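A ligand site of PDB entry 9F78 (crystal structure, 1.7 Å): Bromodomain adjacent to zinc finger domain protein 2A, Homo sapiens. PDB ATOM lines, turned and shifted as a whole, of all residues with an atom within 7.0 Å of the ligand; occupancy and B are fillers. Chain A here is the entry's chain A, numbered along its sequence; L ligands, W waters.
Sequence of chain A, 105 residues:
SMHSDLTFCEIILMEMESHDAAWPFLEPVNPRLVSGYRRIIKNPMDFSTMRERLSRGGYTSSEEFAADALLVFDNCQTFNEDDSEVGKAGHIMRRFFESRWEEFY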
ATOM      1  N   TRP A  23      -0.187  -1.237  -7.072  1.00  0.00           N
ATOM      2  CA  TRP A  23       0.562  -0.466  -8.077  1.00  0.00           C
ATOM      3  C   TRP A  23       0.960  -1.242  -9.336  1.00  0.00           C
ATOM      4  O   TRP A  23       1.031  -0.625 -10.400  1.00  0.00           O
ATOM      5  CB  TRP A  23       1.805   0.182  -7.443  1.00  0.00           C
ATOM      6  CG  TRP A  23       2.786  -0.784  -6.887  1.00  0.00           C
ATOM      7  CD1 TRP A  23       2.857  -1.224  -5.597  1.00  0.00           C
ATOM      8  CD2 TRP A  23       3.850  -1.435  -7.592  1.00  0.00           C
ATOM      9  NE1 TRP A  23       3.888  -2.116  -5.456  1.00  0.00           N
ATOM     10  CE2 TRP A  23       4.520  -2.258  -6.673  1.00  0.00           C
ATOM     11  CE3 TRP A  23       4.297  -1.399  -8.916  1.00  0.00           C
ATOM     12  CZ2 TRP A  23       5.609  -3.053  -7.037  1.00  0.00           C
ATOM     13  CZ3 TRP A  23       5.384  -2.190  -9.270  1.00  0.00           C
ATOM     14  CH2 TRP A  23       6.020  -2.992  -8.335  1.00  0.00           C
ATOM     15  N   PRO A  24       1.197  -2.564  -9.306  1.00  0.00           N
ATOM     16  CA  PRO A  24       1.476  -3.256 -10.567  1.00  0.00           C
ATOM     17  C   PRO A  24       0.241  -3.562 -11.422  1.00  0.00           C
ATOM     18  O   PRO A  24       0.413  -4.027 -12.554  1.00  0.00           O
ATOM     19  CB  PRO A  24       2.143  -4.573 -10.123  1.00  0.00           C
ATOM     20  CG  PRO A  24       2.486  -4.385  -8.665  1.00  0.00           C
ATOM     21  CD  PRO A  24       1.388  -3.485  -8.172  1.00  0.00           C
ATOM     22  N   PHE A  25      -0.969  -3.308 -10.923  1.00  0.00           N
ATOM     23  CA  PHE A  25      -2.165  -3.894 -11.516  1.00  0.00           C
ATOM     24  C   PHE A  25      -3.190  -2.861 -11.967  1.00  0.00           C
ATOM     25  O   PHE A  25      -4.325  -3.238 -12.245  1.00  0.00           O
ATOM     26  CB  PHE A  25      -2.811  -4.876 -10.535  1.00  0.00           C
ATOM     27  CG  PHE A  25      -1.832  -5.858  -9.927  1.00  0.00           C
ATOM     28  CD1 PHE A  25      -1.213  -6.801 -10.738  1.00  0.00           C
ATOM     29  CD2 PHE A  25      -1.512  -5.827  -8.584  1.00  0.00           C
ATOM     30  CE1 PHE A  25      -0.303  -7.698 -10.232  1.00  0.00           C
ATOM     31  CE2 PHE A  25      -0.592  -6.729  -8.050  1.00  0.00           C
ATOM     32  CZ  PHE A  25       0.009  -7.667  -8.868  1.00  0.00           C
ATOM     33  N   LEU A  26      -2.789  -1.585 -12.072  1.00  0.00           N
ATOM     34  CA  LEU A  26      -3.695  -0.484 -12.378  1.00  0.00           C
ATOM     35  C   LEU A  26      -3.812  -0.194 -13.860  1.00  0.00           C
ATOM     36  O   LEU A  26      -4.759   0.496 -14.282  1.00  0.00           O
ATOM     37  CB  LEU A  26      -3.209   0.780 -11.654  1.00  0.00           C
ATOM     38  CG  LEU A  26      -3.170   0.698 -10.129  1.00  0.00           C
ATOM     39  CD1 LEU A  26      -2.609   1.978  -9.529  1.00  0.00           C
ATOM     40  CD2 LEU A  26      -4.544   0.391  -9.541  1.00  0.00           C
ATOM     41  N   GLU A  27      -2.874  -0.690 -14.668  1.00  0.00           N
ATOM     42  CA  GLU A  27      -2.889  -0.486 -16.107  1.00  0.00           C
ATOM     43  C   GLU A  27      -2.335  -1.745 -16.757  1.00  0.00           C
ATOM     44  O   GLU A  27      -1.609  -2.501 -16.103  1.00  0.00           O
ATOM     45  CB  GLU A  27      -2.058   0.753 -16.515  1.00  0.00           C
ATOM     46  CG  GLU A  27      -0.586   0.646 -16.234  1.00  0.00           C
ATOM     47  CD  GLU A  27       0.181   1.843 -16.740  1.00  0.00           C
ATOM     48  OE1 GLU A  27       0.170   2.107 -17.969  1.00  0.00           O
ATOM     49  OE2 GLU A  27       0.802   2.527 -15.911  1.00  0.00           O
ATOM     50  N   PRO A  28      -2.701  -2.013 -18.016  1.00  0.00           N
ATOM     51  CA  PRO A  28      -2.226  -3.239 -18.667  1.00  0.00           C
ATOM     52  C   PRO A  28      -0.718  -3.242 -18.832  1.00  0.00           C
ATOM     53  O   PRO A  28      -0.084  -2.210 -19.059  1.00  0.00           O
ATOM     54  CB  PRO A  28      -2.939  -3.221 -20.021  1.00  0.00           C
ATOM     55  CG  PRO A  28      -4.074  -2.234 -19.881  1.00  0.00           C
ATOM     56  CD  PRO A  28      -3.625  -1.240 -18.864  1.00  0.00           C
ATOM     57  N   VAL A  29      -0.130  -4.435 -18.690  1.00  0.00           N
ATOM     58  CA  VAL A  29       1.251  -4.647 -19.085  1.00  0.00           C
ATOM     59  C   VAL A  29       1.353  -4.385 -20.578  1.00  0.00           C
ATOM     60  O   VAL A  29       0.573  -4.940 -21.360  1.00  0.00           O
ATOM     61  CB  VAL A  29       1.682  -6.083 -18.750  1.00  0.00           C
ATOM     62  CG1 VAL A  29       3.116  -6.346 -19.232  1.00  0.00           C
ATOM     63  CG2 VAL A  29       1.514  -6.368 -17.276  1.00  0.00           C
ATOM     64  N   ASN A  30       2.309  -3.552 -20.982  1.00  0.00           N
ATOM     65  CA  ASN A  30       2.502  -3.307 -22.410  1.00  0.00           C
ATOM     66  C   ASN A  30       3.442  -4.365 -22.961  1.00  0.00           C
ATOM     67  O   ASN A  30       4.660  -4.302 -22.700  1.00  0.00           O
ATOM     68  CB  ASN A  30       3.071  -1.914 -22.660  1.00  0.00           C
ATOM     69  CG  ASN A  30       3.008  -1.540 -24.133  1.00  0.00           C
ATOM     70  OD1 ASN A  30       3.173  -2.384 -25.016  1.00  0.00           O
ATOM     71  ND2 ASN A  30       2.739  -0.263 -24.400  1.00  0.00           N
ATOM     72  N   PRO A  31       2.949  -5.334 -23.730  1.00  0.00           N
ATOM     73  CA  PRO A  31       3.807  -6.459 -24.149  1.00  0.00           C
ATOM     74  C   PRO A  31       5.057  -6.045 -24.908  1.00  0.00           C
ATOM     75  O   PRO A  31       6.059  -6.758 -24.845  1.00  0.00           O
ATOM     76  CB  PRO A  31       2.863  -7.303 -25.011  1.00  0.00           C
ATOM     77  CG  PRO A  31       1.773  -6.366 -25.424  1.00  0.00           C
ATOM     78  CD  PRO A  31       1.588  -5.436 -24.282  1.00  0.00           C
ATOM     79  N   ARG A  32       5.023  -4.883 -25.581  1.00  0.00           N
ATOM     80  CA  ARG A  32       6.190  -4.408 -26.366  1.00  0.00           C
ATOM     81  C   ARG A  32       7.300  -3.917 -25.424  1.00  0.00           C
ATOM     82  O   ARG A  32       8.470  -3.898 -25.844  1.00  0.00           O
ATOM     83  CB  ARG A  32       5.761  -3.271 -27.298  1.00  0.00           C
ATOM     84  CG  ARG A  32       6.102  -3.491 -28.769  1.00  0.00           C
ATOM     85  CD  ARG A  32       5.643  -2.345 -29.646  1.00  0.00           C
ATOM     86  NE  ARG A  32       4.706  -2.783 -30.680  1.00  0.00           N
ATOM     87  CZ  ARG A  32       3.385  -2.657 -30.591  1.00  0.00           C
ATOM     88  NH1 ARG A  32       2.839  -2.113 -29.524  1.00  0.00           N
ATOM     89  NH2 ARG A  32       2.621  -3.083 -31.575  1.00  0.00           N
ATOM     90  N   LEU A  33       6.943  -3.565 -24.187  1.00  0.00           N
ATOM     91  CA  LEU A  33       7.877  -3.001 -23.222  1.00  0.00           C
ATOM     92  C   LEU A  33       8.427  -4.035 -22.238  1.00  0.00           C
ATOM     93  O   LEU A  33       9.277  -3.695 -21.396  1.00  0.00           O
ATOM     94  CB  LEU A  33       7.189  -1.863 -22.461  1.00  0.00           C
ATOM     95  CG  LEU A  33       7.315  -0.455 -23.047  1.00  0.00           C
ATOM     96  CD1 LEU A  33       6.757  -0.377 -24.467  1.00  0.00           C
ATOM     97  CD2 LEU A  33       6.615   0.553 -22.151  1.00  0.00           C
ATOM     98  N   VAL A  34       7.998  -5.288 -22.330  1.00  0.00           N
ATOM     99  CA  VAL A  34       8.400  -6.335 -21.401  1.00  0.00           C
ATOM    100  C   VAL A  34       8.786  -7.543 -22.241  1.00  0.00           C
ATOM    101  O   VAL A  34       7.921  -8.193 -22.845  1.00  0.00           O
ATOM    102  CB  VAL A  34       7.309  -6.708 -20.394  1.00  0.00           C
ATOM    103  CG1 VAL A  34       7.794  -7.829 -19.477  1.00  0.00           C
ATOM    104  CG2 VAL A  34       6.884  -5.466 -19.602  1.00  0.00           C
ATOM    105  N   TYR A  37       6.716 -11.197 -22.396  1.00  0.00           N
ATOM    106  CA  TYR A  37       5.404 -11.212 -21.778  1.00  0.00           C
ATOM    107  C   TYR A  37       4.341 -11.770 -22.722  1.00  0.00           C
ATOM    108  O   TYR A  37       3.510 -12.601 -22.321  1.00  0.00           O
ATOM    109  CB  TYR A  37       5.016  -9.812 -21.308  1.00  0.00           C
ATOM    110  CG  TYR A  37       3.845  -9.836 -20.345  1.00  0.00           C
ATOM    111  CD1 TYR A  37       4.010 -10.277 -19.042  1.00  0.00           C
ATOM    112  CD2 TYR A  37       2.560  -9.455 -20.758  1.00  0.00           C
ATOM    113  CE1 TYR A  37       2.964 -10.325 -18.160  1.00  0.00           C
ATOM    114  CE2 TYR A  37       1.496  -9.498 -19.884  1.00  0.00           C
ATOM    115  CZ  TYR A  37       1.686  -9.926 -18.579  1.00  0.00           C
ATOM    116  OH  TYR A  37       0.670  -9.989 -17.672  1.00  0.00           O
ATOM    117  N   ILE A  41       2.029 -14.984 -21.470  1.00  0.00           N
ATOM    118  CA  ILE A  41       0.709 -14.634 -20.930  1.00  0.00           C
ATOM    119  C   ILE A  41      -0.237 -14.458 -22.111  1.00  0.00           C
ATOM    120  O   ILE A  41      -0.128 -13.487 -22.863  1.00  0.00           O
ATOM    121  CB  ILE A  41       0.765 -13.368 -20.070  1.00  0.00           C
ATOM    122  CG1 ILE A  41       1.683 -13.586 -18.878  1.00  0.00           C
ATOM    123  CG2 ILE A  41      -0.643 -13.016 -19.531  1.00  0.00           C
ATOM    124  CD1 ILE A  41       1.183 -14.671 -17.948  1.00  0.00           C
ATOM    125  N   MET A  45      -4.746  -9.409 -18.007  1.00  0.00           N
ATOM    126  CA  MET A  45      -5.812  -8.789 -17.231  1.00  0.00           C
ATOM    127  C   MET A  45      -5.196  -7.815 -16.230  1.00  0.00           C
ATOM    128  O   MET A  45      -4.069  -8.004 -15.753  1.00  0.00           O
ATOM    129  CB  MET A  45      -6.675  -9.838 -16.513  1.00  0.00           C
ATOM    130  CG  MET A  45      -7.961  -9.291 -15.885  1.00  0.00           C
ATOM    131  SD  MET A  45      -8.929  -8.213 -16.962  1.00  0.00           S
ATOM    132  CE  MET A  45      -9.265  -9.282 -18.356  1.00  0.00           C
ATOM    133  N   VAL A  72      -5.527 -11.810 -13.052  1.00  0.00           N
ATOM    134  CA  VAL A  72      -4.516 -10.823 -12.712  1.00  0.00           C
ATOM    135  C   VAL A  72      -3.433 -11.454 -11.853  1.00  0.00           C
ATOM    136  O   VAL A  72      -2.239 -11.303 -12.123  1.00  0.00           O
ATOM    137  CB  VAL A  72      -5.144  -9.611 -11.992  1.00  0.00           C
ATOM    138  CG1 VAL A  72      -4.076  -8.597 -11.637  1.00  0.00           C
ATOM    139  CG2 VAL A  72      -6.184  -8.986 -12.882  1.00  0.00           C
ATOM    140  N   ASN A  75      -1.626 -14.640 -13.764  1.00  0.00           N
ATOM    141  CA  ASN A  75      -0.628 -14.117 -14.682  1.00  0.00           C
ATOM    142  C   ASN A  75       0.600 -13.625 -13.925  1.00  0.00           C
ATOM    143  O   ASN A  75       1.740 -13.838 -14.359  1.00  0.00           O
ATOM    144  CB  ASN A  75      -1.199 -12.970 -15.498  1.00  0.00           C
ATOM    145  CG  ASN A  75      -2.221 -13.432 -16.475  1.00  0.00           C
ATOM    146  OD1 ASN A  75      -2.288 -14.617 -16.788  1.00  0.00           O
ATOM    147  ND2 ASN A  75      -3.045 -12.501 -16.975  1.00  0.00           N
ATOM    148  N   CYS A  76       0.378 -12.945 -12.791  1.00  0.00           N
ATOM    149  CA  CYS A  76       1.498 -12.358 -12.059  1.00  0.00           C
ATOM    150  C   CYS A  76       2.389 -13.433 -11.466  1.00  0.00           C
ATOM    151  O   CYS A  76       3.624 -13.305 -11.488  1.00  0.00           O
ATOM    152  CB  CYS A  76       0.970 -11.413 -10.967  1.00  0.00           C
ATOM    153  SG  CYS A  76       2.278 -10.669  -9.943  1.00  0.00           S
ATOM    154  N   PHE A  79       4.579 -15.273 -14.354  1.00  0.00           N
ATOM    155  CA  PHE A  79       5.620 -14.529 -15.045  1.00  0.00           C
ATOM    156  C   PHE A  79       6.671 -13.928 -14.124  1.00  0.00           C
ATOM    157  O   PHE A  79       7.778 -13.647 -14.588  1.00  0.00           O
ATOM    158  CB  PHE A  79       4.992 -13.395 -15.869  1.00  0.00           C
ATOM    159  CG  PHE A  79       5.964 -12.656 -16.757  1.00  0.00           C
ATOM    160  CD1 PHE A  79       6.534 -11.459 -16.354  1.00  0.00           C
ATOM    161  CD2 PHE A  79       6.310 -13.180 -18.009  1.00  0.00           C
ATOM    162  CE1 PHE A  79       7.412 -10.775 -17.185  1.00  0.00           C
ATOM    163  CE2 PHE A  79       7.203 -12.509 -18.830  1.00  0.00           C
ATOM    164  CZ  PHE A  79       7.737 -11.305 -18.417  1.00  0.00           C
ATOM    165  N   ASN A  80       6.360 -13.741 -12.844  1.00  0.00           N
ATOM    166  CA  ASN A  80       7.241 -13.050 -11.906  1.00  0.00           C
ATOM    167  C   ASN A  80       7.639 -13.946 -10.741  1.00  0.00           C
ATOM    168  O   ASN A  80       6.838 -14.748 -10.255  1.00  0.00           O
ATOM    169  CB  ASN A  80       6.571 -11.788 -11.355  1.00  0.00           C
ATOM    170  CG  ASN A  80       6.187 -10.813 -12.439  1.00  0.00           C
ATOM    171  OD1 ASN A  80       7.037 -10.108 -12.981  1.00  0.00           O
ATOM    172  ND2 ASN A  80       4.895 -10.748 -12.755  1.00  0.00           N
ATOM    173  N   VAL A  86       6.979  -7.088  -7.917  1.00  0.00           N
ATOM    174  CA  VAL A  86       5.682  -7.348  -8.549  1.00  0.00           C
ATOM    175  C   VAL A  86       5.124  -8.700  -8.100  1.00  0.00           C
ATOM    176  O   VAL A  86       3.928  -8.817  -7.800  1.00  0.00           O
ATOM    177  CB  VAL A  86       5.798  -7.262 -10.070  1.00  0.00           C
ATOM    178  CG1 VAL A  86       4.522  -7.789 -10.756  1.00  0.00           C
ATOM    179  CG2 VAL A  86       6.066  -5.818 -10.478  1.00  0.00           C
HETATM  180  C1  LIG L   1       8.157  -1.784 -17.577  1.00  0.00           C
HETATM  181  C2  LIG L   1       7.524  -1.460 -18.936  1.00  0.00           C
HETATM  182  C3  LIG L   1       6.002  -1.341 -18.851  1.00  0.00           C
HETATM  183  C4  LIG L   1       3.987  -0.738 -18.334  1.00  0.00           C
HETATM  184  C5  LIG L   1       2.772  -0.014 -17.701  1.00  0.00           C
HETATM  185  C6  LIG L   1       2.216  -1.769 -16.469  1.00  0.00           C
HETATM  186  C7  LIG L   1       2.105  -2.299 -15.038  1.00  0.00           C
HETATM  187  C8  LIG L   1       3.392  -0.551 -14.239  1.00  0.00           C
HETATM  188  C9  LIG L   1       3.563   0.000 -15.665  1.00  0.00           C
HETATM  189  C10 LIG L   1       4.208  -2.930 -13.714  1.00  0.00           C
HETATM  190  C11 LIG L   1       3.866  -4.436 -13.906  1.00  0.00           C
HETATM  191  C12 LIG L   1       2.761  -6.316 -13.842  1.00  0.00           C
HETATM  192  C13 LIG L   1       1.663  -7.349 -13.564  1.00  0.00           C
HETATM  193  C14 LIG L   1       3.947  -6.558 -14.500  1.00  0.00           C
HETATM  194  C15 LIG L   1       4.371  -7.913 -15.060  1.00  0.00           C
HETATM  195  C16 LIG L   1       5.537  -7.990 -16.057  1.00  0.00           C
HETATM  196  C17 LIG L   1       4.651  -5.377 -14.540  1.00  0.00           C
HETATM  197  C18 LIG L   1       6.029  -5.141 -15.162  1.00  0.00           C
HETATM  198  C19 LIG L   1       6.050  -3.971 -16.141  1.00  0.00           C
HETATM  199  N1  LIG L   1       5.293  -0.485 -18.103  1.00  0.00           N
HETATM  200  N2  LIG L   1       2.554  -0.415 -16.525  1.00  0.00           N
HETATM  201  N3  LIG L   1       3.261  -1.950 -14.291  1.00  0.00           N
HETATM  202  N4  LIG L   1       2.741  -5.015 -13.503  1.00  0.00           N
HETATM  203  N5  LIG L   1       3.920  -1.721 -19.213  1.00  0.00           N
HETATM  204  O1  LIG L   1       5.170  -2.575 -13.121  1.00  0.00           O
HETATM  205  O2  LIG L   1       3.784  -8.885 -14.735  1.00  0.00           O
HETATM  206  O3  LIG L   1       5.158  -2.081 -19.521  1.00  0.00           O
HETATM  207  O   HOH W   1       5.839   2.715 -17.084  1.00  0.00           O
HETATM  208  O   HOH W   2      -0.831  -9.640 -13.726  1.00  0.00           O
HETATM  209  O   HOH W   3       1.444 -10.276 -15.075  1.00  0.00           O
HETATM  210  O   HOH W   4       7.633  -2.903 -12.125  1.00  0.00           O
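The side-chain sulfur (SG) of Cys 76 is in hydrogen-bond range of the backbone carbonyl oxygen (O) of Val 86. The backbone carbonyl oxygen of Cys 76 lies within hydrogen-bond range of the side-chain amide nitrogen of Asn 80 (3.1 Å). N of Arg 32 lies close to OD1 of Asn 30, 3.2 Å away.
The backbone carbonyl oxygen (O) of Pro 24 lies within hydrogen-bond range of a nitrogen (N4) of the ligand. A nitrogen (N2) of the ligand lies within salt-bridge range of the side-chain carboxylate of Glu 27 (3.5 Å). N of Asn 30 lies within hydrogen-bond range of N5 of the ligand. The side-chain amide nitrogen (ND2) of Asn 80 sits at hydrogen-bond distance from an oxygen (O2) of the ligand, at 2.9 Å.
Water W3 bridges OH of Tyr 37 (2.7 Å) and O2 of the ligand (2.7 Å).
Merely in contact with the ligand: Pro 28, Phe 79, Leu 33, Val 29, Val 34, Tyr 37, Val 86, Trp 23 and Phe 25. Hydrophobic or aromatic side chains that line the ligand: Trp 23, Pro 24, Phe 25, Val 29, Leu 33, Val 34, Tyr 37, Phe 79 and Val 86.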
